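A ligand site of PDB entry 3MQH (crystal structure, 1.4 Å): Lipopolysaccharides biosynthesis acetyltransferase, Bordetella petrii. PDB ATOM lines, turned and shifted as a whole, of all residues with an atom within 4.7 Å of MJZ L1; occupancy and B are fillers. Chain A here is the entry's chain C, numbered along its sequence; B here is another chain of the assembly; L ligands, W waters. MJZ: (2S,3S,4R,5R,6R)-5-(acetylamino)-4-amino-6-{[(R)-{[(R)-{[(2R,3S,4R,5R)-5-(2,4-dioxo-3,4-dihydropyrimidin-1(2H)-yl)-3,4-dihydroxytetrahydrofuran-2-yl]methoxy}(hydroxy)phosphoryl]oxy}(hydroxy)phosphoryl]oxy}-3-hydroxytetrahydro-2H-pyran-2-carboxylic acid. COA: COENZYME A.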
ATOM      1  N   HIS A  29      33.001 -11.865  25.209  1.00  0.00           N
ATOM      2  CA  HIS A  29      31.659 -11.300  25.188  1.00  0.00           C
ATOM      3  C   HIS A  29      30.645 -12.395  24.901  1.00  0.00           C
ATOM      4  O   HIS A  29      30.708 -13.052  23.846  1.00  0.00           O
ATOM      5  CB  HIS A  29      31.530 -10.153  24.183  1.00  0.00           C
ATOM      6  CG  HIS A  29      30.118  -9.697  24.014  1.00  0.00           C
ATOM      7  ND1 HIS A  29      29.602  -9.350  22.790  1.00  0.00           N
ATOM      8  CD2 HIS A  29      29.118  -9.543  24.912  1.00  0.00           C
ATOM      9  CE1 HIS A  29      28.333  -8.987  22.931  1.00  0.00           C
ATOM     10  NE2 HIS A  29      28.015  -9.120  24.206  1.00  0.00           N
ATOM     11  N   CYS A  31      26.506 -13.022  24.552  1.00  0.00           N
ATOM     12  CA  CYS A  31      25.211 -12.353  24.354  1.00  0.00           C
ATOM     13  C   CYS A  31      24.146 -12.941  25.285  1.00  0.00           C
ATOM     14  O   CYS A  31      24.256 -14.070  25.814  1.00  0.00           O
ATOM     15  CB  CYS A  31      24.765 -12.401  22.882  1.00  0.00           C
ATOM     16  SG  CYS A  31      25.859 -11.462  21.795  1.00  0.00           S
ATOM     17  N   PHE A  47      33.728 -15.120  21.580  1.00  0.00           N
ATOM     18  CA  PHE A  47      32.448 -14.464  21.396  1.00  0.00           C
ATOM     19  C   PHE A  47      31.401 -15.545  21.361  1.00  0.00           C
ATOM     20  O   PHE A  47      31.612 -16.608  20.776  1.00  0.00           O
ATOM     21  CB  PHE A  47      32.394 -13.757  20.028  1.00  0.00           C
ATOM     22  CG  PHE A  47      31.015 -13.277  19.676  1.00  0.00           C
ATOM     23  CD1 PHE A  47      30.489 -12.170  20.324  1.00  0.00           C
ATOM     24  CD2 PHE A  47      30.231 -13.959  18.771  1.00  0.00           C
ATOM     25  CE1 PHE A  47      29.179 -11.725  20.036  1.00  0.00           C
ATOM     26  CE2 PHE A  47      28.930 -13.556  18.491  1.00  0.00           C
ATOM     27  CZ  PHE A  47      28.380 -12.415  19.146  1.00  0.00           C
ATOM     28  N   ASN A  50      23.554 -15.086  20.521  1.00  0.00           N
ATOM     29  CA  ASN A  50      22.324 -15.323  21.266  1.00  0.00           C
ATOM     30  C   ASN A  50      21.727 -16.679  21.007  1.00  0.00           C
ATOM     31  O   ASN A  50      21.288 -17.314  21.956  1.00  0.00           O
ATOM     32  CB  ASN A  50      21.282 -14.290  20.852  1.00  0.00           C
ATOM     33  CG  ASN A  50      21.569 -12.909  21.433  1.00  0.00           C
ATOM     34  OD1 ASN A  50      21.599 -12.736  22.659  1.00  0.00           O
ATOM     35  ND2 ASN A  50      21.795 -11.938  20.554  1.00  0.00           N
ATOM     36  N   TYR A  67      28.945 -18.385  16.880  1.00  0.00           N
ATOM     37  CA  TYR A  67      27.909 -17.534  16.319  1.00  0.00           C
ATOM     38  C   TYR A  67      26.528 -18.184  16.498  1.00  0.00           C
ATOM     39  O   TYR A  67      26.353 -19.380  16.723  1.00  0.00           O
ATOM     40  CB  TYR A  67      28.186 -17.362  14.820  1.00  0.00           C
ATOM     41  CG  TYR A  67      29.369 -16.459  14.559  1.00  0.00           C
ATOM     42  CD1 TYR A  67      29.369 -15.138  15.011  1.00  0.00           C
ATOM     43  CD2 TYR A  67      30.479 -16.904  13.825  1.00  0.00           C
ATOM     44  CE1 TYR A  67      30.445 -14.270  14.764  1.00  0.00           C
ATOM     45  CE2 TYR A  67      31.531 -16.044  13.604  1.00  0.00           C
ATOM     46  CZ  TYR A  67      31.514 -14.760  14.048  1.00  0.00           C
ATOM     47  OH  TYR A  67      32.571 -13.895  13.763  1.00  0.00           O
ATOM     48  N   ASN A  86      27.784 -19.046   9.881  1.00  0.00           N
ATOM     49  CA  ASN A  86      26.329 -19.311   9.863  1.00  0.00           C
ATOM     50  C   ASN A  86      25.683 -18.907   8.537  1.00  0.00           C
ATOM     51  O   ASN A  86      24.534 -19.256   8.340  1.00  0.00           O
ATOM     52  CB  ASN A  86      25.551 -18.693  11.046  1.00  0.00           C
ATOM     53  CG  ASN A  86      25.778 -17.230  11.259  1.00  0.00           C
ATOM     54  OD1 ASN A  86      26.134 -16.514  10.331  1.00  0.00           O
ATOM     55  ND2 ASN A  86      25.527 -16.749  12.500  1.00  0.00           N
ATOM     56  N   VAL A  87      26.387 -18.237   7.627  1.00  0.00           N
ATOM     57  CA  VAL A  87      25.835 -18.004   6.278  1.00  0.00           C
ATOM     58  C   VAL A  87      26.727 -18.716   5.248  1.00  0.00           C
ATOM     59  O   VAL A  87      27.960 -18.580   5.265  1.00  0.00           O
ATOM     60  CB  VAL A  87      25.703 -16.507   5.964  1.00  0.00           C
ATOM     61  CG1 VAL A  87      25.313 -16.281   4.475  1.00  0.00           C
ATOM     62  CG2 VAL A  87      24.617 -15.891   6.873  1.00  0.00           C
ATOM     63  N   PRO A  90      27.817 -15.668   1.849  1.00  0.00           N
ATOM     64  CA  PRO A  90      27.552 -14.303   2.254  1.00  0.00           C
ATOM     65  C   PRO A  90      27.896 -13.297   1.148  1.00  0.00           C
ATOM     66  O   PRO A  90      28.854 -13.491   0.384  1.00  0.00           O
ATOM     67  CB  PRO A  90      28.480 -14.103   3.467  1.00  0.00           C
ATOM     68  CG  PRO A  90      29.548 -15.140   3.319  1.00  0.00           C
ATOM     69  CD  PRO A  90      28.788 -16.335   2.734  1.00  0.00           C
ATOM     70  N   ILE A  94      23.529  -8.217   0.564  1.00  0.00           N
ATOM     71  CA  ILE A  94      22.328  -9.049   0.663  1.00  0.00           C
ATOM     72  C   ILE A  94      22.252  -9.600   2.079  1.00  0.00           C
ATOM     73  O   ILE A  94      22.886 -10.593   2.437  1.00  0.00           O
ATOM     74  CB  ILE A  94      22.349 -10.182  -0.339  1.00  0.00           C
ATOM     75  CG1 ILE A  94      22.518  -9.617  -1.752  1.00  0.00           C
ATOM     76  CG2 ILE A  94      21.055 -10.987  -0.278  1.00  0.00           C
ATOM     77  CD1 ILE A  94      22.770 -10.715  -2.797  1.00  0.00           C
ATOM     78  N   GLU A  95      21.496  -8.969   2.961  1.00  0.00           N
ATOM     79  CA  GLU A  95      21.387  -9.461   4.317  1.00  0.00           C
ATOM     80  C   GLU A  95      20.792 -10.863   4.351  1.00  0.00           C
ATOM     81  O   GLU A  95      19.782 -11.176   3.701  1.00  0.00           O
ATOM     82  CB  GLU A  95      20.532  -8.451   5.087  1.00  0.00           C
ATOM     83  CG  GLU A  95      20.641  -8.582   6.584  1.00  0.00           C
ATOM     84  CD  GLU A  95      19.303  -8.953   7.153  1.00  0.00           C
ATOM     85  OE1 GLU A  95      18.787 -10.004   6.717  1.00  0.00           O
ATOM     86  OE2 GLU A  95      18.814  -8.177   8.001  1.00  0.00           O
ATOM     87  N   ARG A  96      21.446 -11.778   5.072  1.00  0.00           N
ATOM     88  CA  ARG A  96      21.061 -13.188   5.062  1.00  0.00           C
ATOM     89  C   ARG A  96      20.763 -13.727   6.462  1.00  0.00           C
ATOM     90  O   ARG A  96      20.913 -14.919   6.753  1.00  0.00           O
ATOM     91  CB  ARG A  96      22.039 -14.090   4.296  1.00  0.00           C
ATOM     92  CG  ARG A  96      21.882 -13.921   2.773  1.00  0.00           C
ATOM     93  CD  ARG A  96      22.768 -14.889   1.937  1.00  0.00           C
ATOM     94  NE  ARG A  96      22.139 -14.937   0.612  1.00  0.00           N
ATOM     95  CZ  ARG A  96      22.703 -14.583  -0.539  1.00  0.00           C
ATOM     96  NH1 ARG A  96      23.973 -14.201  -0.645  1.00  0.00           N
ATOM     97  NH2 ARG A  96      21.960 -14.610  -1.629  1.00  0.00           N
ATOM     98  N   LYS A  97      20.321 -12.820   7.319  1.00  0.00           N
ATOM     99  CA  LYS A  97      20.025 -13.203   8.686  1.00  0.00           C
ATOM    100  C   LYS A  97      18.891 -14.214   8.805  1.00  0.00           C
ATOM    101  O   LYS A  97      18.836 -14.928   9.796  1.00  0.00           O
ATOM    102  CB  LYS A  97      19.846 -11.999   9.599  1.00  0.00           C
ATOM    103  CG  LYS A  97      21.134 -11.202   9.747  1.00  0.00           C
ATOM    104  CD  LYS A  97      21.036 -10.225  10.905  1.00  0.00           C
ATOM    105  CE  LYS A  97      22.434  -9.855  11.390  1.00  0.00           C
ATOM    106  NZ  LYS A  97      22.411  -9.054  12.634  1.00  0.00           N
ATOM    107  N   TYR A 100      20.380 -18.311   7.967  1.00  0.00           N
ATOM    108  CA  TYR A 100      21.405 -19.043   8.716  1.00  0.00           C
ATOM    109  C   TYR A 100      21.244 -20.553   8.642  1.00  0.00           C
ATOM    110  O   TYR A 100      20.128 -21.113   8.636  1.00  0.00           O
ATOM    111  CB  TYR A 100      21.405 -18.594  10.176  1.00  0.00           C
ATOM    112  CG  TYR A 100      21.886 -17.216  10.482  1.00  0.00           C
ATOM    113  CD1 TYR A 100      22.379 -16.343   9.523  1.00  0.00           C
ATOM    114  CD2 TYR A 100      21.841 -16.776  11.801  1.00  0.00           C
ATOM    115  CE1 TYR A 100      22.831 -15.066   9.856  1.00  0.00           C
ATOM    116  CE2 TYR A 100      22.280 -15.492  12.132  1.00  0.00           C
ATOM    117  CZ  TYR A 100      22.768 -14.648  11.168  1.00  0.00           C
ATOM    118  OH  TYR A 100      23.215 -13.378  11.506  1.00  0.00           O
ATOM    119  N   ARG B  23      28.837   0.871  12.472  1.00  0.00           N
ATOM    120  CA  ARG B  23      28.701   0.249  13.799  1.00  0.00           C
ATOM    121  C   ARG B  23      30.033  -0.390  14.159  1.00  0.00           C
ATOM    122  O   ARG B  23      30.549  -1.246  13.393  1.00  0.00           O
ATOM    123  CB  ARG B  23      27.612  -0.803  13.861  1.00  0.00           C
ATOM    124  CG  ARG B  23      26.224  -0.186  13.593  1.00  0.00           C
ATOM    125  CD  ARG B  23      25.075  -1.216  13.599  1.00  0.00           C
ATOM    126  NE  ARG B  23      25.166  -2.274  12.588  1.00  0.00           N
ATOM    127  CZ  ARG B  23      25.281  -2.114  11.276  1.00  0.00           C
ATOM    128  NH1 ARG B  23      25.341  -0.910  10.706  1.00  0.00           N
ATOM    129  NH2 ARG B  23      25.336  -3.187  10.493  1.00  0.00           N
ATOM    130  N   TRP B  25      32.140  -2.438  17.080  1.00  0.00           N
ATOM    131  CA  TRP B  25      31.833  -3.313  18.207  1.00  0.00           C
ATOM    132  C   TRP B  25      32.931  -3.441  19.249  1.00  0.00           C
ATOM    133  O   TRP B  25      33.851  -2.622  19.331  1.00  0.00           O
ATOM    134  CB  TRP B  25      31.268  -4.655  17.695  1.00  0.00           C
ATOM    135  CG  TRP B  25      29.887  -4.460  17.088  1.00  0.00           C
ATOM    136  CD1 TRP B  25      29.578  -4.295  15.753  1.00  0.00           C
ATOM    137  CD2 TRP B  25      28.642  -4.402  17.788  1.00  0.00           C
ATOM    138  NE1 TRP B  25      28.206  -4.140  15.604  1.00  0.00           N
ATOM    139  CE2 TRP B  25      27.618  -4.223  16.838  1.00  0.00           C
ATOM    140  CE3 TRP B  25      28.286  -4.499  19.157  1.00  0.00           C
ATOM    141  CZ2 TRP B  25      26.272  -4.127  17.190  1.00  0.00           C
ATOM    142  CZ3 TRP B  25      26.943  -4.431  19.510  1.00  0.00           C
ATOM    143  CH2 TRP B  25      25.964  -4.236  18.525  1.00  0.00           C
ATOM    144  N   HIS B  26      32.850  -4.496  20.057  1.00  0.00           N
ATOM    145  CA  HIS B  26      33.633  -4.554  21.291  1.00  0.00           C
ATOM    146  C   HIS B  26      35.125  -4.652  21.019  1.00  0.00           C
ATOM    147  O   HIS B  26      35.563  -5.467  20.170  1.00  0.00           O
ATOM    148  CB  HIS B  26      33.234  -5.728  22.183  1.00  0.00           C
ATOM    149  CG  HIS B  26      31.768  -5.812  22.492  1.00  0.00           C
ATOM    150  ND1 HIS B  26      30.793  -5.992  21.529  1.00  0.00           N
ATOM    151  CD2 HIS B  26      31.114  -5.766  23.679  1.00  0.00           C
ATOM    152  CE1 HIS B  26      29.611  -6.026  22.101  1.00  0.00           C
ATOM    153  NE2 HIS B  26      29.778  -5.905  23.408  1.00  0.00           N
ATOM    154  N   SER B  41      30.146  -2.287   9.225  1.00  0.00           N
ATOM    155  CA  SER B  41      30.092  -2.991  10.490  1.00  0.00           C
ATOM    156  C   SER B  41      31.419  -3.603  10.807  1.00  0.00           C
ATOM    157  O   SER B  41      31.969  -4.346   9.979  1.00  0.00           O
ATOM    158  CB  SER B  41      28.966  -4.033  10.517  1.00  0.00           C
ATOM    159  OG  SER B  41      28.991  -4.724  11.770  1.00  0.00           O
ATOM    160  N   GLY B  43      33.288  -6.050  13.558  1.00  0.00           N
ATOM    161  CA  GLY B  43      33.034  -6.885  14.726  1.00  0.00           C
ATOM    162  C   GLY B  43      34.099  -6.885  15.818  1.00  0.00           C
ATOM    163  O   GLY B  43      35.101  -6.158  15.751  1.00  0.00           O
ATOM    164  N   GLN B  44      33.876  -7.767  16.800  1.00  0.00           N
ATOM    165  CA  GLN B  44      34.710  -7.830  17.994  1.00  0.00           C
ATOM    166  C   GLN B  44      36.180  -7.925  17.614  1.00  0.00           C
ATOM    167  O   GLN B  44      36.527  -8.754  16.746  1.00  0.00           O
ATOM    168  CB  GLN B  44      34.283  -9.007  18.859  1.00  0.00           C
ATOM    169  CG  GLN B  44      35.077  -9.234  20.098  1.00  0.00           C
ATOM    170  CD  GLN B  44      34.427 -10.255  20.990  1.00  0.00           C
ATOM    171  OE1 GLN B  44      33.236 -10.207  21.273  1.00  0.00           O
ATOM    172  NE2 GLN B  44      35.216 -11.205  21.458  1.00  0.00           N
ATOM    173  N   LYS B  59      31.102  -5.111   5.484  1.00  0.00           N
ATOM    174  CA  LYS B  59      30.817  -5.883   6.693  1.00  0.00           C
ATOM    175  C   LYS B  59      32.020  -6.715   7.062  1.00  0.00           C
ATOM    176  O   LYS B  59      32.438  -7.592   6.300  1.00  0.00           O
ATOM    177  CB  LYS B  59      29.599  -6.784   6.482  1.00  0.00           C
ATOM    178  CG  LYS B  59      28.294  -5.974   6.279  1.00  0.00           C
ATOM    179  CD  LYS B  59      27.075  -6.892   6.173  1.00  0.00           C
ATOM    180  CE  LYS B  59      25.853  -6.071   5.738  1.00  0.00           C
ATOM    181  NZ  LYS B  59      24.656  -6.916   5.470  1.00  0.00           N
ATOM    182  N   GLN B  61      33.661  -9.132   9.889  1.00  0.00           N
ATOM    183  CA  GLN B  61      33.355  -9.986  11.026  1.00  0.00           C
ATOM    184  C   GLN B  61      34.479  -9.977  12.069  1.00  0.00           C
ATOM    185  O   GLN B  61      35.545  -9.378  11.863  1.00  0.00           O
ATOM    186  CB  GLN B  61      33.009 -11.403  10.555  1.00  0.00           C
ATOM    187  CG  GLN B  61      31.854 -11.470   9.521  1.00  0.00           C
ATOM    188  CD  GLN B  61      30.621 -10.655   9.924  1.00  0.00           C
ATOM    189  OE1 GLN B  61      30.106 -10.750  11.053  1.00  0.00           O
ATOM    190  NE2 GLN B  61      30.128  -9.865   8.961  1.00  0.00           N
ATOM    191  N   ASN B  62      34.222 -10.658  13.181  1.00  0.00           N
ATOM    192  CA  ASN B  62      35.188 -10.680  14.277  1.00  0.00           C
ATOM    193  C   ASN B  62      36.623 -11.027  13.845  1.00  0.00           C
ATOM    194  O   ASN B  62      36.829 -11.860  12.950  1.00  0.00           O
ATOM    195  CB  ASN B  62      34.783 -11.699  15.334  1.00  0.00           C
ATOM    196  CG  ASN B  62      33.467 -11.362  16.035  1.00  0.00           C
ATOM    197  OD1 ASN B  62      32.868 -10.327  15.780  1.00  0.00           O
ATOM    198  ND2 ASN B  62      33.019 -12.278  16.878  1.00  0.00           N
ATOM    199  N   PHE B  77      32.633  -8.112   1.828  1.00  0.00           N
ATOM    200  CA  PHE B  77      32.339  -8.892   3.018  1.00  0.00           C
ATOM    201  C   PHE B  77      33.635  -9.559   3.461  1.00  0.00           C
ATOM    202  O   PHE B  77      34.246 -10.317   2.701  1.00  0.00           O
ATOM    203  CB  PHE B  77      31.287  -9.963   2.696  1.00  0.00           C
ATOM    204  CG  PHE B  77      30.842 -10.739   3.898  1.00  0.00           C
ATOM    205  CD1 PHE B  77      29.695 -10.347   4.606  1.00  0.00           C
ATOM    206  CD2 PHE B  77      31.532 -11.881   4.345  1.00  0.00           C
ATOM    207  CE1 PHE B  77      29.238 -11.055   5.741  1.00  0.00           C
ATOM    208  CE2 PHE B  77      31.074 -12.575   5.479  1.00  0.00           C
ATOM    209  CZ  PHE B  77      29.963 -12.167   6.162  1.00  0.00           C
HETATM  210  N1  MJZ L   1      27.171  -7.767  17.992  1.00  0.00           N
HETATM  211  C2  MJZ L   1      26.959  -7.948  19.308  1.00  0.00           C
HETATM  212  O2  MJZ L   1      27.927  -8.123  20.070  1.00  0.00           O
HETATM  213  N3  MJZ L   1      25.686  -7.976  19.814  1.00  0.00           N
HETATM  214  C4  MJZ L   1      24.627  -7.781  18.986  1.00  0.00           C
HETATM  215  O4  MJZ L   1      23.463  -7.803  19.479  1.00  0.00           O
HETATM  216  C5  MJZ L   1      24.816  -7.546  17.631  1.00  0.00           C
HETATM  217  C6  MJZ L   1      26.139  -7.549  17.162  1.00  0.00           C
HETATM  218  PA  MJZ L   1      26.131  -8.361  13.065  1.00  0.00           P
HETATM  219  PB  MJZ L   1      26.796  -8.545  10.155  1.00  0.00           P
HETATM  220  O'P MJZ L   1      23.903 -11.061   6.459  1.00  0.00           O
HETATM  221  O'Q MJZ L   1      25.316 -12.539   5.591  1.00  0.00           O
HETATM  222  C1' MJZ L   1      25.770 -10.981  10.069  1.00  0.00           C
HETATM  223  O1A MJZ L   1      25.734  -6.925  13.122  1.00  0.00           O
HETATM  224  O1B MJZ L   1      25.440  -7.971   9.799  1.00  0.00           O
HETATM  225  C1C MJZ L   1      28.575  -7.705  17.563  1.00  0.00           C
HETATM  226  C2' MJZ L   1      26.382 -12.290  10.543  1.00  0.00           C
HETATM  227  N2' MJZ L   1      27.211 -12.028  11.723  1.00  0.00           N
HETATM  228  O2A MJZ L   1      25.036  -9.350  13.113  1.00  0.00           O
HETATM  229  O2B MJZ L   1      28.054  -7.965   9.633  1.00  0.00           O
HETATM  230  C2C MJZ L   1      29.289  -9.060  17.557  1.00  0.00           C
HETATM  231  O2C MJZ L   1      30.672  -8.868  17.846  1.00  0.00           O
HETATM  232  C3' MJZ L   1      27.199 -12.940   9.425  1.00  0.00           C
HETATM  233  N3' MJZ L   1      27.664 -14.301   9.914  1.00  0.00           N
HETATM  234  O3A MJZ L   1      27.026  -8.607  11.750  1.00  0.00           O
HETATM  235  O3B MJZ L   1      26.840 -10.080   9.768  1.00  0.00           O
HETATM  236  C3C MJZ L   1      29.129  -9.519  16.120  1.00  0.00           C
HETATM  237  O3C MJZ L   1      30.168 -10.416  15.783  1.00  0.00           O
HETATM  238  C4' MJZ L   1      26.312 -13.095   8.194  1.00  0.00           C
HETATM  239  O4' MJZ L   1      27.161 -13.654   7.149  1.00  0.00           O
HETATM  240  C4C MJZ L   1      29.249  -8.226  15.347  1.00  0.00           C
HETATM  241  O4C MJZ L   1      28.579  -7.285  16.193  1.00  0.00           O
HETATM  242  C5' MJZ L   1      25.804 -11.741   7.752  1.00  0.00           C
HETATM  243  O5' MJZ L   1      25.065 -11.123   8.835  1.00  0.00           O
HETATM  244  C5C MJZ L   1      28.533  -8.245  14.009  1.00  0.00           C
HETATM  245  O5C MJZ L   1      27.194  -8.751  14.172  1.00  0.00           O
HETATM  246  C6' MJZ L   1      24.933 -11.782   6.520  1.00  0.00           C
HETATM  247  C7' MJZ L   1      27.048 -12.701  12.865  1.00  0.00           C
HETATM  248  O7' MJZ L   1      26.326 -13.683  12.987  1.00  0.00           O
HETATM  249  C8' MJZ L   1      27.821 -12.180  14.047  1.00  0.00           C
HETATM  250  N1A COA L   2      37.466 -25.097   0.570  1.00  0.00           N
HETATM  251  C2A COA L   2      37.888 -26.103  -0.212  1.00  0.00           C
HETATM  252  N3A COA L   2      37.092 -26.721  -1.097  1.00  0.00           N
HETATM  253  C4A COA L   2      35.826 -26.338  -1.208  1.00  0.00           C
HETATM  254  C5A COA L   2      35.308 -25.253  -0.377  1.00  0.00           C
HETATM  255  C6A COA L   2      36.236 -24.609   0.556  1.00  0.00           C
HETATM  256  N6A COA L   2      35.833 -23.595   1.347  1.00  0.00           N
HETATM  257  N7A COA L   2      34.022 -25.049  -0.708  1.00  0.00           N
HETATM  258  C8A COA L   2      33.710 -25.942  -1.678  1.00  0.00           C
HETATM  259  N9A COA L   2      34.791 -26.707  -1.971  1.00  0.00           N
HETATM  260  C1B COA L   2      34.895 -27.785  -2.980  1.00  0.00           C
HETATM  261  C2B COA L   2      33.865 -28.854  -2.686  1.00  0.00           C
HETATM  262  O2B COA L   2      34.425 -29.840  -1.802  1.00  0.00           O
HETATM  263  C3B COA L   2      33.605 -29.347  -4.102  1.00  0.00           C
HETATM  264  O3B COA L   2      34.704 -30.157  -4.496  1.00  0.00           O
HETATM  265  P3B COA L   2      34.736 -31.772  -4.311  1.00  0.00           P
HETATM  266  O7A COA L   2      36.071 -32.113  -4.945  1.00  0.00           O
HETATM  267  O8A COA L   2      33.550 -32.211  -5.142  1.00  0.00           O
HETATM  268  O9A COA L   2      34.553 -32.188  -2.857  1.00  0.00           O
HETATM  269  C4B COA L   2      33.634 -28.076  -4.923  1.00  0.00           C
HETATM  270  O4B COA L   2      34.482 -27.176  -4.195  1.00  0.00           O
HETATM  271  C5B COA L   2      32.279 -27.419  -5.130  1.00  0.00           C
HETATM  272  O5B COA L   2      31.663 -27.360  -3.839  1.00  0.00           O
HETATM  273  P1A COA L   2      30.132 -26.963  -3.645  1.00  0.00           P
HETATM  274  O1A COA L   2      29.838 -27.180  -2.182  1.00  0.00           O
HETATM  275  O2A COA L   2      29.307 -27.710  -4.689  1.00  0.00           O
HETATM  276  O3A COA L   2      30.123 -25.417  -4.035  1.00  0.00           O
HETATM  277  P2A COA L   2      29.079 -24.239  -3.752  1.00  0.00           P
HETATM  278  O4A COA L   2      27.907 -24.748  -3.009  1.00  0.00           O
HETATM  279  O5A COA L   2      28.841 -23.586  -5.083  1.00  0.00           O
HETATM  280  O6A COA L   2      29.924 -23.179  -2.923  1.00  0.00           O
HETATM  281  CBP COA L   2      30.975 -22.382  -0.901  1.00  0.00           C
HETATM  282  CCP COA L   2      30.368 -23.598  -1.615  1.00  0.00           C
HETATM  283  CDP COA L   2      30.025 -21.184  -0.850  1.00  0.00           C
HETATM  284  CEP COA L   2      32.290 -21.959  -1.568  1.00  0.00           C
HETATM  285  CAP COA L   2      31.166 -22.756   0.579  1.00  0.00           C
HETATM  286  OAP COA L   2      31.860 -24.032   0.644  1.00  0.00           O
HETATM  287  C9P COA L   2      31.991 -21.784   1.367  1.00  0.00           C
HETATM  288  O9P COA L   2      33.223 -21.817   1.417  1.00  0.00           O
HETATM  289  N8P COA L   2      31.275 -20.867   2.031  1.00  0.00           N
HETATM  290  C7P COA L   2      31.829 -19.785   2.858  1.00  0.00           C
HETATM  291  C6P COA L   2      31.076 -19.670   4.185  1.00  0.00           C
HETATM  292  C5P COA L   2      31.637 -18.506   4.923  1.00  0.00           C
HETATM  293  O5P COA L   2      32.843 -18.224   4.908  1.00  0.00           O
HETATM  294  N4P COA L   2      30.771 -17.754   5.616  1.00  0.00           N
HETATM  295  C3P COA L   2      31.308 -16.619   6.368  1.00  0.00           C
HETATM  296  C2P COA L   2      30.121 -15.844   6.960  1.00  0.00           C
HETATM  297  S1P COA L   2      29.412 -16.563   8.490  1.00  0.00           S
HETATM  298  O   HOH W   1      21.165  -7.886  17.843  1.00  0.00           O
HETATM  299  O   HOH W   2      22.308  -9.263  21.586  1.00  0.00           O
HETATM  300  O   HOH W   3      25.267  -9.380   4.372  1.00  0.00           O
HETATM  301  O   HOH W   4      26.016 -14.559  15.712  1.00  0.00           O
HETATM  302  O   HOH W   5      26.726  -4.493  13.156  1.00  0.00           O
HETATM  303  O   HOH W   6      31.178  -8.710  20.521  1.00  0.00           O
HETATM  304  O   HOH W   7      24.456  -5.601  10.166  1.00  0.00           O
HETATM  305  O   HOH W   8      30.209  -7.093  11.391  1.00  0.00           O
HETATM  306  O   HOH W   9      30.212 -14.514  10.929  1.00  0.00           O
HETATM  307  O   HOH W  10      23.807  -8.502   7.806  1.00  0.00           O
HETATM  308  O   HOH W  11      25.322  -7.486  22.580  1.00  0.00           O
HETATM  309  O   HOH W  12      24.863 -12.468   2.895  1.00  0.00           O
HETATM  310  O   HOH W  13      23.666  -5.926  14.581  1.00  0.00           O
HETATM  311  O   HOH W  14      31.357 -11.389  13.398  1.00  0.00           O
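Water W7 bridges the guanidinium group of Arg 23 of chain B and an oxygen (O1B) of MJZ L1.
Water W5 lies within hydrogen-bond range of O1A of MJZ L1 (2.6 Å), OG of Ser 41 of chain B (2.7 Å), NE of Arg 23 of chain B (2.8 Å) and NE1 of Trp 25 of chain B (2.9 Å).
Water W9 lies within hydrogen-bond range of a nitrogen (N3') of MJZ L1 (2.8 Å) and a sulfur (S1P) of COA L2 (3.3 Å).
Water W2 bridges O4 of MJZ L1 and ND2 of Asn 50.
Water W8 lies within hydrogen-bond range of the side-chain hydroxyl of Ser 41 of chain B (2.7 Å) and an oxygen (O2B) of MJZ L1 (2.9 Å).
Water W3 lies within hydrogen-bond range of NZ of Lys 59 of chain B (2.8 Å), O'P of MJZ L1 (3.0 Å) and O of Ile 94 (3.3 Å).
The backbone NH (N) of Gln 44 of chain B lies within hydrogen-bond range of the side-chain amide oxygen (OD1) of Asn 62 of chain B (2.9 Å).
The backbone NH (N) of Lys 97 sits at hydrogen-bond distance from the side-chain carboxylate (OE1) of Glu 95, at 3.3 Å.
The indole nitrogen of Trp 25 of chain B lies close to an oxygen (O4C) of MJZ L1, 3.2 Å away.
The side-chain amino group (NZ) of Lys 97 is in salt-bridge range of an oxygen (O2A) of MJZ L1 (2.7 Å).
OD1 of Asn 86 sits at hydrogen-bond distance from N3' of MJZ L1 (2.7 Å).
S1P of COA L2 lies close to OD1 of Asn 86 (3.8 Å).
O3C of MJZ L1 lies within hydrogen-bond range of OD1 of Asn 62 of chain B (2.7 Å).
ND1 of His 29 lies close to O2 of MJZ L1, 3.4 Å away.
N4P of COA L2 is in hydrogen-bond range of O of Val 87.
The side-chain hydroxyl (OH) of Tyr 100 sits at hydrogen-bond distance from an oxygen (O7') of MJZ L1 (3.5 Å).
The backbone NH of Asn 86 sits close to a sulfur (S1P) of COA L2 (3.3 Å).
N of Val 87 sits close to S1P of COA L2.
NE2 of Gln 61 of chain B sits at hydrogen-bond distance from O2B of MJZ L1.
The backbone NH (N) of Arg 96 sits at hydrogen-bond distance from an oxygen (O'P) of MJZ L1 (2.9 Å).
N3' of MJZ L1 sits close to S1P of COA L2 (3.2 Å).
Residues that only touch MJZ L1: Phe 47, Tyr 67, Val 87, Pro 90, Glu 95, His 26 of chain B, Ser 41 of chain B, Gln 44 of chain B, Lys 59 of chain B and Phe 77 of chain B.
Hydrophobic or aromatic side chains that line MJZ L1: His 29, Phe 47, Tyr 67, Val 87, Pro 90, Trp 25 of chain B, His 26 of chain B and Phe 77 of chain B.
Of the 23 residues printed, 18 come within 4 Å of MJZ L1.
Along chain A the residues within 4 Å of MJZ L1 span positions 29 to 100.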
